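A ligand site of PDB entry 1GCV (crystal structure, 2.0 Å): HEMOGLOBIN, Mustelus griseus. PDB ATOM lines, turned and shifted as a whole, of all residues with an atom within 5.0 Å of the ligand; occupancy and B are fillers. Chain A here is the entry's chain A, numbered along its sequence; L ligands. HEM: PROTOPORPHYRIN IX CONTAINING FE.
NE2 of His 87 binds FE of the ligand (2.2 Å). NZ of Lys 61 is in salt-bridge range of O1A of the ligand (3.8 Å).
Merely in contact with the ligand: Tyr 42 (3.9 Å), Phe 43 (3.8 Å), His 58 (3.5 Å), Val 62 (3.8 Å), Ala 65 (3.8 Å), Leu 83 (3.7 Å), Leu 91 (3.3 Å), Val 93 (3.5 Å), Asn 97 (3.7 Å), Phe 98 (3.7 Å), Leu 101 (3.5 Å) and Leu 135 (3.7 Å). Hydrophobic or aromatic side chains that line the ligand: Tyr 42, Phe 43, Val 62, Ala 65, Leu 83, His 87, Leu 91, Val 93, Phe 98, Leu 101 and Leu 135. Of the 20 residues printed, 14 come within 4 Å of the ligand.
The backbone carbonyl oxygen (O) of Thr 86 lies within hydrogen-bond range of the backbone NH (N) of Leu 91 (2.7 Å). ND1 of His 87 is in hydrogen-bond range of O of Leu 83 (3.0 Å). O of His 87 is in hydrogen-bond range of N of Val 93 (3.3 Å).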
ATOM      1  N   LEU A  32      -7.528  -9.358 -10.016  1.00  0.00           N
ATOM      2  CA  LEU A  32      -6.331  -8.706  -9.484  1.00  0.00           C
ATOM      3  C   LEU A  32      -5.977  -7.490 -10.324  1.00  0.00           C
ATOM      4  O   LEU A  32      -5.649  -6.430  -9.788  1.00  0.00           O
ATOM      5  CB  LEU A  32      -5.145  -9.686  -9.486  1.00  0.00           C
ATOM      6  CG  LEU A  32      -3.779  -9.119  -9.086  1.00  0.00           C
ATOM      7  CD1 LEU A  32      -3.727  -8.867  -7.596  1.00  0.00           C
ATOM      8  CD2 LEU A  32      -2.677 -10.098  -9.500  1.00  0.00           C
ATOM      9  N   SER A  39      -0.299  -4.279 -10.472  1.00  0.00           N
ATOM     10  CA  SER A  39       0.179  -5.619 -10.754  1.00  0.00           C
ATOM     11  C   SER A  39       0.245  -5.922 -12.246  1.00  0.00           C
ATOM     12  O   SER A  39       0.850  -6.904 -12.656  1.00  0.00           O
ATOM     13  CB  SER A  39      -0.696  -6.658 -10.034  1.00  0.00           C
ATOM     14  OG  SER A  39      -2.009  -6.683 -10.562  1.00  0.00           O
ATOM     15  N   TYR A  42       3.852  -6.272 -14.489  1.00  0.00           N
ATOM     16  CA  TYR A  42       4.723  -7.408 -14.771  1.00  0.00           C
ATOM     17  C   TYR A  42       4.409  -8.125 -16.068  1.00  0.00           C
ATOM     18  O   TYR A  42       5.232  -8.912 -16.562  1.00  0.00           O
ATOM     19  CB  TYR A  42       4.646  -8.434 -13.641  1.00  0.00           C
ATOM     20  CG  TYR A  42       5.147  -7.898 -12.342  1.00  0.00           C
ATOM     21  CD1 TYR A  42       6.499  -7.991 -12.011  1.00  0.00           C
ATOM     22  CD2 TYR A  42       4.288  -7.261 -11.460  1.00  0.00           C
ATOM     23  CE1 TYR A  42       6.982  -7.446 -10.821  1.00  0.00           C
ATOM     24  CE2 TYR A  42       4.746  -6.712 -10.272  1.00  0.00           C
ATOM     25  CZ  TYR A  42       6.095  -6.811  -9.962  1.00  0.00           C
ATOM     26  OH  TYR A  42       6.548  -6.257  -8.789  1.00  0.00           O
ATOM     27  N   PHE A  43       3.230  -7.860 -16.620  1.00  0.00           N
ATOM     28  CA  PHE A  43       2.797  -8.518 -17.837  1.00  0.00           C
ATOM     29  C   PHE A  43       2.572  -7.587 -19.007  1.00  0.00           C
ATOM     30  O   PHE A  43       1.937  -6.541 -18.879  1.00  0.00           O
ATOM     31  CB  PHE A  43       1.504  -9.284 -17.554  1.00  0.00           C
ATOM     32  CG  PHE A  43       1.495  -9.974 -16.222  1.00  0.00           C
ATOM     33  CD1 PHE A  43       1.056  -9.307 -15.081  1.00  0.00           C
ATOM     34  CD2 PHE A  43       1.955 -11.278 -16.102  1.00  0.00           C
ATOM     35  CE1 PHE A  43       1.076  -9.934 -13.843  1.00  0.00           C
ATOM     36  CE2 PHE A  43       1.983 -11.912 -14.877  1.00  0.00           C
ATOM     37  CZ  PHE A  43       1.537 -11.239 -13.737  1.00  0.00           C
ATOM     38  N   HIS A  58      -1.349 -18.051 -18.254  1.00  0.00           N
ATOM     39  CA  HIS A  58      -0.718 -17.733 -16.977  1.00  0.00           C
ATOM     40  C   HIS A  58      -1.628 -18.133 -15.822  1.00  0.00           C
ATOM     41  O   HIS A  58      -1.182 -18.686 -14.823  1.00  0.00           O
ATOM     42  CB  HIS A  58      -0.396 -16.240 -16.909  1.00  0.00           C
ATOM     43  CG  HIS A  58       0.422 -15.890 -15.697  1.00  0.00           C
ATOM     44  ND1 HIS A  58       0.057 -14.921 -14.764  1.00  0.00           N
ATOM     45  CD2 HIS A  58       1.553 -16.598 -15.305  1.00  0.00           C
ATOM     46  CE1 HIS A  58       0.936 -15.065 -13.765  1.00  0.00           C
ATOM     47  NE2 HIS A  58       1.794 -15.995 -14.058  1.00  0.00           N
ATOM     48  N   LYS A  61      -1.190 -21.720 -15.254  1.00  0.00           N
ATOM     49  CA  LYS A  61       0.079 -22.100 -14.625  1.00  0.00           C
ATOM     50  C   LYS A  61      -0.022 -21.861 -13.117  1.00  0.00           C
ATOM     51  O   LYS A  61       0.467 -22.660 -12.317  1.00  0.00           O
ATOM     52  CB  LYS A  61       1.215 -21.258 -15.179  1.00  0.00           C
ATOM     53  CG  LYS A  61       1.864 -21.788 -16.438  1.00  0.00           C
ATOM     54  CD  LYS A  61       3.042 -20.922 -16.813  1.00  0.00           C
ATOM     55  CE  LYS A  61       3.454 -21.113 -18.263  1.00  0.00           C
ATOM     56  NZ  LYS A  61       4.808 -20.538 -18.489  1.00  0.00           N
ATOM     57  N   VAL A  62      -0.649 -20.760 -12.744  1.00  0.00           N
ATOM     58  CA  VAL A  62      -0.812 -20.395 -11.339  1.00  0.00           C
ATOM     59  C   VAL A  62      -1.691 -21.374 -10.566  1.00  0.00           C
ATOM     60  O   VAL A  62      -1.330 -21.830  -9.479  1.00  0.00           O
ATOM     61  CB  VAL A  62      -1.398 -18.971 -11.198  1.00  0.00           C
ATOM     62  CG1 VAL A  62      -1.787 -18.695  -9.743  1.00  0.00           C
ATOM     63  CG2 VAL A  62      -0.377 -17.947 -11.671  1.00  0.00           C
ATOM     64  N   ALA A  65      -0.201 -24.852 -10.049  1.00  0.00           N
ATOM     65  CA  ALA A  65       0.782 -24.816  -8.972  1.00  0.00           C
ATOM     66  C   ALA A  65       0.083 -24.829  -7.613  1.00  0.00           C
ATOM     67  O   ALA A  65       0.598 -25.386  -6.651  1.00  0.00           O
ATOM     68  CB  ALA A  65       1.676 -23.587  -9.095  1.00  0.00           C
ATOM     69  N   VAL A  66      -1.094 -24.215  -7.557  1.00  0.00           N
ATOM     70  CA  VAL A  66      -1.874 -24.169  -6.321  1.00  0.00           C
ATOM     71  C   VAL A  66      -2.404 -25.574  -6.040  1.00  0.00           C
ATOM     72  O   VAL A  66      -2.328 -26.067  -4.910  1.00  0.00           O
ATOM     73  CB  VAL A  66      -3.058 -23.159  -6.441  1.00  0.00           C
ATOM     74  CG1 VAL A  66      -4.040 -23.358  -5.302  1.00  0.00           C
ATOM     75  CG2 VAL A  66      -2.547 -21.735  -6.434  1.00  0.00           C
ATOM     76  N   LEU A  83       9.718 -23.017  -7.170  1.00  0.00           N
ATOM     77  CA  LEU A  83       8.829 -21.907  -7.499  1.00  0.00           C
ATOM     78  C   LEU A  83       9.235 -20.656  -6.710  1.00  0.00           C
ATOM     79  O   LEU A  83       9.097 -19.543  -7.208  1.00  0.00           O
ATOM     80  CB  LEU A  83       7.379 -22.279  -7.191  1.00  0.00           C
ATOM     81  CG  LEU A  83       6.262 -21.612  -8.006  1.00  0.00           C
ATOM     82  CD1 LEU A  83       6.663 -21.522  -9.470  1.00  0.00           C
ATOM     83  CD2 LEU A  83       4.990 -22.434  -7.861  1.00  0.00           C
ATOM     84  N   THR A  86      12.277 -19.102  -8.371  1.00  0.00           N
ATOM     85  CA  THR A  86      11.895 -18.439  -9.618  1.00  0.00           C
ATOM     86  C   THR A  86      11.364 -17.009  -9.444  1.00  0.00           C
ATOM     87  O   THR A  86      11.728 -16.113 -10.211  1.00  0.00           O
ATOM     88  CB  THR A  86      10.822 -19.238 -10.374  1.00  0.00           C
ATOM     89  OG1 THR A  86      11.330 -20.548 -10.684  1.00  0.00           O
ATOM     90  CG2 THR A  86      10.436 -18.542 -11.674  1.00  0.00           C
ATOM     91  N   HIS A  87      10.511 -16.794  -8.449  1.00  0.00           N
ATOM     92  CA  HIS A  87       9.948 -15.461  -8.195  1.00  0.00           C
ATOM     93  C   HIS A  87      10.959 -14.534  -7.528  1.00  0.00           C
ATOM     94  O   HIS A  87      11.073 -13.350  -7.881  1.00  0.00           O
ATOM     95  CB  HIS A  87       8.708 -15.560  -7.315  1.00  0.00           C
ATOM     96  CG  HIS A  87       7.501 -16.034  -8.090  1.00  0.00           C
ATOM     97  ND1 HIS A  87       7.350 -17.391  -8.293  1.00  0.00           N
ATOM     98  CD2 HIS A  87       6.518 -15.273  -8.722  1.00  0.00           C
ATOM     99  CE1 HIS A  87       6.265 -17.467  -9.070  1.00  0.00           C
ATOM    100  NE2 HIS A  87       5.770 -16.309  -9.335  1.00  0.00           N
ATOM    101  N   LEU A  91      12.218 -13.816 -11.575  1.00  0.00           N
ATOM    102  CA  LEU A  91      11.143 -12.873 -11.875  1.00  0.00           C
ATOM    103  C   LEU A  91      11.210 -11.598 -11.043  1.00  0.00           C
ATOM    104  O   LEU A  91      10.806 -10.529 -11.502  1.00  0.00           O
ATOM    105  CB  LEU A  91       9.783 -13.547 -11.680  1.00  0.00           C
ATOM    106  CG  LEU A  91       9.585 -14.827 -12.486  1.00  0.00           C
ATOM    107  CD1 LEU A  91       8.332 -15.510 -12.012  1.00  0.00           C
ATOM    108  CD2 LEU A  91       9.506 -14.534 -13.976  1.00  0.00           C
ATOM    109  N   VAL A  93       9.481 -10.544  -8.517  1.00  0.00           N
ATOM    110  CA  VAL A  93       8.150  -9.973  -8.308  1.00  0.00           C
ATOM    111  C   VAL A  93       8.075  -9.449  -6.869  1.00  0.00           C
ATOM    112  O   VAL A  93       8.406 -10.164  -5.928  1.00  0.00           O
ATOM    113  CB  VAL A  93       7.063 -11.054  -8.505  1.00  0.00           C
ATOM    114  CG1 VAL A  93       5.694 -10.491  -8.156  1.00  0.00           C
ATOM    115  CG2 VAL A  93       7.097 -11.561  -9.933  1.00  0.00           C
ATOM    116  N   ASN A  97       2.665  -8.351  -3.689  1.00  0.00           N
ATOM    117  CA  ASN A  97       1.612  -8.752  -4.612  1.00  0.00           C
ATOM    118  C   ASN A  97       0.963 -10.105  -4.300  1.00  0.00           C
ATOM    119  O   ASN A  97      -0.211 -10.303  -4.596  1.00  0.00           O
ATOM    120  CB  ASN A  97       2.143  -8.783  -6.046  1.00  0.00           C
ATOM    121  CG  ASN A  97       2.383  -7.403  -6.611  1.00  0.00           C
ATOM    122  OD1 ASN A  97       3.517  -6.945  -6.700  1.00  0.00           O
ATOM    123  ND2 ASN A  97       1.311  -6.738  -7.018  1.00  0.00           N
ATOM    124  N   PHE A  98       1.735 -11.026  -3.712  1.00  0.00           N
ATOM    125  CA  PHE A  98       1.220 -12.368  -3.405  1.00  0.00           C
ATOM    126  C   PHE A  98      -0.093 -12.368  -2.641  1.00  0.00           C
ATOM    127  O   PHE A  98      -1.042 -13.020  -3.068  1.00  0.00           O
ATOM    128  CB  PHE A  98       2.288 -13.170  -2.665  1.00  0.00           C
ATOM    129  CG  PHE A  98       3.507 -13.458  -3.499  1.00  0.00           C
ATOM    130  CD1 PHE A  98       3.394 -13.802  -4.841  1.00  0.00           C
ATOM    131  CD2 PHE A  98       4.794 -13.341  -2.957  1.00  0.00           C
ATOM    132  CE1 PHE A  98       4.526 -14.029  -5.629  1.00  0.00           C
ATOM    133  CE2 PHE A  98       5.919 -13.562  -3.745  1.00  0.00           C
ATOM    134  CZ  PHE A  98       5.780 -13.902  -5.075  1.00  0.00           C
ATOM    135  N   LEU A 101      -3.155 -11.325  -4.728  1.00  0.00           N
ATOM    136  CA  LEU A 101      -3.690 -12.370  -5.587  1.00  0.00           C
ATOM    137  C   LEU A 101      -4.450 -13.421  -4.772  1.00  0.00           C
ATOM    138  O   LEU A 101      -5.406 -13.999  -5.253  1.00  0.00           O
ATOM    139  CB  LEU A 101      -2.574 -13.044  -6.383  1.00  0.00           C
ATOM    140  CG  LEU A 101      -2.973 -14.252  -7.237  1.00  0.00           C
ATOM    141  CD1 LEU A 101      -3.907 -13.814  -8.361  1.00  0.00           C
ATOM    142  CD2 LEU A 101      -1.724 -14.901  -7.811  1.00  0.00           C
ATOM    143  N   ILE A 105      -8.282 -15.005  -5.480  1.00  0.00           N
ATOM    144  CA  ILE A 105      -8.539 -16.428  -5.653  1.00  0.00           C
ATOM    145  C   ILE A 105      -9.721 -16.755  -4.743  1.00  0.00           C
ATOM    146  O   ILE A 105     -10.618 -17.505  -5.111  1.00  0.00           O
ATOM    147  CB  ILE A 105      -7.322 -17.303  -5.224  1.00  0.00           C
ATOM    148  CG1 ILE A 105      -6.222 -17.263  -6.297  1.00  0.00           C
ATOM    149  CG2 ILE A 105      -7.754 -18.759  -5.004  1.00  0.00           C
ATOM    150  CD1 ILE A 105      -4.868 -17.746  -5.806  1.00  0.00           C
ATOM    151  N   ILE A 131       1.439 -20.677   1.199  1.00  0.00           N
ATOM    152  CA  ILE A 131       2.034 -20.655  -0.133  1.00  0.00           C
ATOM    153  C   ILE A 131       2.695 -19.295  -0.373  1.00  0.00           C
ATOM    154  O   ILE A 131       3.791 -19.235  -0.929  1.00  0.00           O
ATOM    155  CB  ILE A 131       0.959 -20.895  -1.221  1.00  0.00           C
ATOM    156  CG1 ILE A 131       0.614 -22.385  -1.290  1.00  0.00           C
ATOM    157  CG2 ILE A 131       1.461 -20.430  -2.574  1.00  0.00           C
ATOM    158  CD1 ILE A 131      -0.603 -22.674  -2.146  1.00  0.00           C
ATOM    159  N   LEU A 135       6.743 -18.548  -1.156  1.00  0.00           N
ATOM    160  CA  LEU A 135       7.079 -17.798  -2.365  1.00  0.00           C
ATOM    161  C   LEU A 135       7.849 -16.504  -2.090  1.00  0.00           C
ATOM    162  O   LEU A 135       8.520 -15.985  -2.971  1.00  0.00           O
ATOM    163  CB  LEU A 135       5.811 -17.483  -3.154  1.00  0.00           C
ATOM    164  CG  LEU A 135       5.471 -18.352  -4.375  1.00  0.00           C
ATOM    165  CD1 LEU A 135       5.876 -19.802  -4.125  1.00  0.00           C
ATOM    166  CD2 LEU A 135       3.986 -18.263  -4.652  1.00  0.00           C
HETATM  167  CHA HEM L   1       5.344 -17.271 -13.349  1.00  0.00           C
HETATM  168  CHB HEM L   1       2.874 -19.477  -9.780  1.00  0.00           C
HETATM  169  CHC HEM L   1       1.813 -15.096  -7.872  1.00  0.00           C
HETATM  170  CHD HEM L   1       4.106 -12.917 -11.538  1.00  0.00           C
HETATM  171  C1A HEM L   1       4.781 -18.254 -12.508  1.00  0.00           C
HETATM  172  C2A HEM L   1       4.743 -19.676 -12.784  1.00  0.00           C
HETATM  173  C3A HEM L   1       4.021 -20.284 -11.831  1.00  0.00           C
HETATM  174  C4A HEM L   1       3.613 -19.246 -10.926  1.00  0.00           C
HETATM  175  CMA HEM L   1       3.758 -21.788 -11.688  1.00  0.00           C
HETATM  176  CAA HEM L   1       5.428 -20.387 -13.924  1.00  0.00           C
HETATM  177  CBA HEM L   1       6.907 -20.364 -13.646  1.00  0.00           C
HETATM  178  CGA HEM L   1       7.716 -20.929 -14.791  1.00  0.00           C
HETATM  179  O1A HEM L   1       7.552 -20.460 -15.934  1.00  0.00           O
HETATM  180  O2A HEM L   1       8.528 -21.850 -14.534  1.00  0.00           O
HETATM  181  C1B HEM L   1       2.433 -18.465  -8.919  1.00  0.00           C
HETATM  182  C2B HEM L   1       1.610 -18.707  -7.729  1.00  0.00           C
HETATM  183  C3B HEM L   1       1.339 -17.478  -7.163  1.00  0.00           C
HETATM  184  C4B HEM L   1       1.979 -16.488  -8.026  1.00  0.00           C
HETATM  185  CMB HEM L   1       1.211 -20.085  -7.183  1.00  0.00           C
HETATM  186  CAB HEM L   1       0.658 -17.226  -5.964  1.00  0.00           C
HETATM  187  CBB HEM L   1      -0.596 -17.769  -5.654  1.00  0.00           C
HETATM  188  C1C HEM L   1       2.324 -14.142  -8.729  1.00  0.00           C
HETATM  189  C2C HEM L   1       2.002 -12.720  -8.645  1.00  0.00           C
HETATM  190  C3C HEM L   1       2.682 -12.109  -9.672  1.00  0.00           C
HETATM  191  C4C HEM L   1       3.379 -13.150 -10.384  1.00  0.00           C
HETATM  192  CMC HEM L   1       1.053 -12.089  -7.635  1.00  0.00           C
HETATM  193  CAC HEM L   1       2.776 -10.763  -9.984  1.00  0.00           C
HETATM  194  CBC HEM L   1       1.706  -9.859 -10.048  1.00  0.00           C
HETATM  195  C1D HEM L   1       4.697 -13.916 -12.303  1.00  0.00           C
HETATM  196  C2D HEM L   1       5.384 -13.634 -13.540  1.00  0.00           C
HETATM  197  C3D HEM L   1       5.679 -14.848 -14.063  1.00  0.00           C
HETATM  198  C4D HEM L   1       5.218 -15.888 -13.141  1.00  0.00           C
HETATM  199  CMD HEM L   1       5.741 -12.264 -14.125  1.00  0.00           C
HETATM  200  CAD HEM L   1       6.353 -15.052 -15.406  1.00  0.00           C
HETATM  201  CBD HEM L   1       5.269 -15.208 -16.457  1.00  0.00           C
HETATM  202  CGD HEM L   1       5.813 -15.784 -17.757  1.00  0.00           C
HETATM  203  O1D HEM L   1       6.851 -16.475 -17.713  1.00  0.00           O
HETATM  204  O2D HEM L   1       5.186 -15.536 -18.805  1.00  0.00           O
HETATM  205  NA  HEM L   1       4.085 -17.977 -11.333  1.00  0.00           N
HETATM  206  NB  HEM L   1       2.696 -17.096  -9.084  1.00  0.00           N
HETATM  207  NC  HEM L   1       3.173 -14.418  -9.814  1.00  0.00           N
HETATM  208  ND  HEM L   1       4.630 -15.296 -12.022  1.00  0.00           N
HETATM  209 FE   HEM L   1       3.875 -16.207 -10.412  1.00  0.00          FE
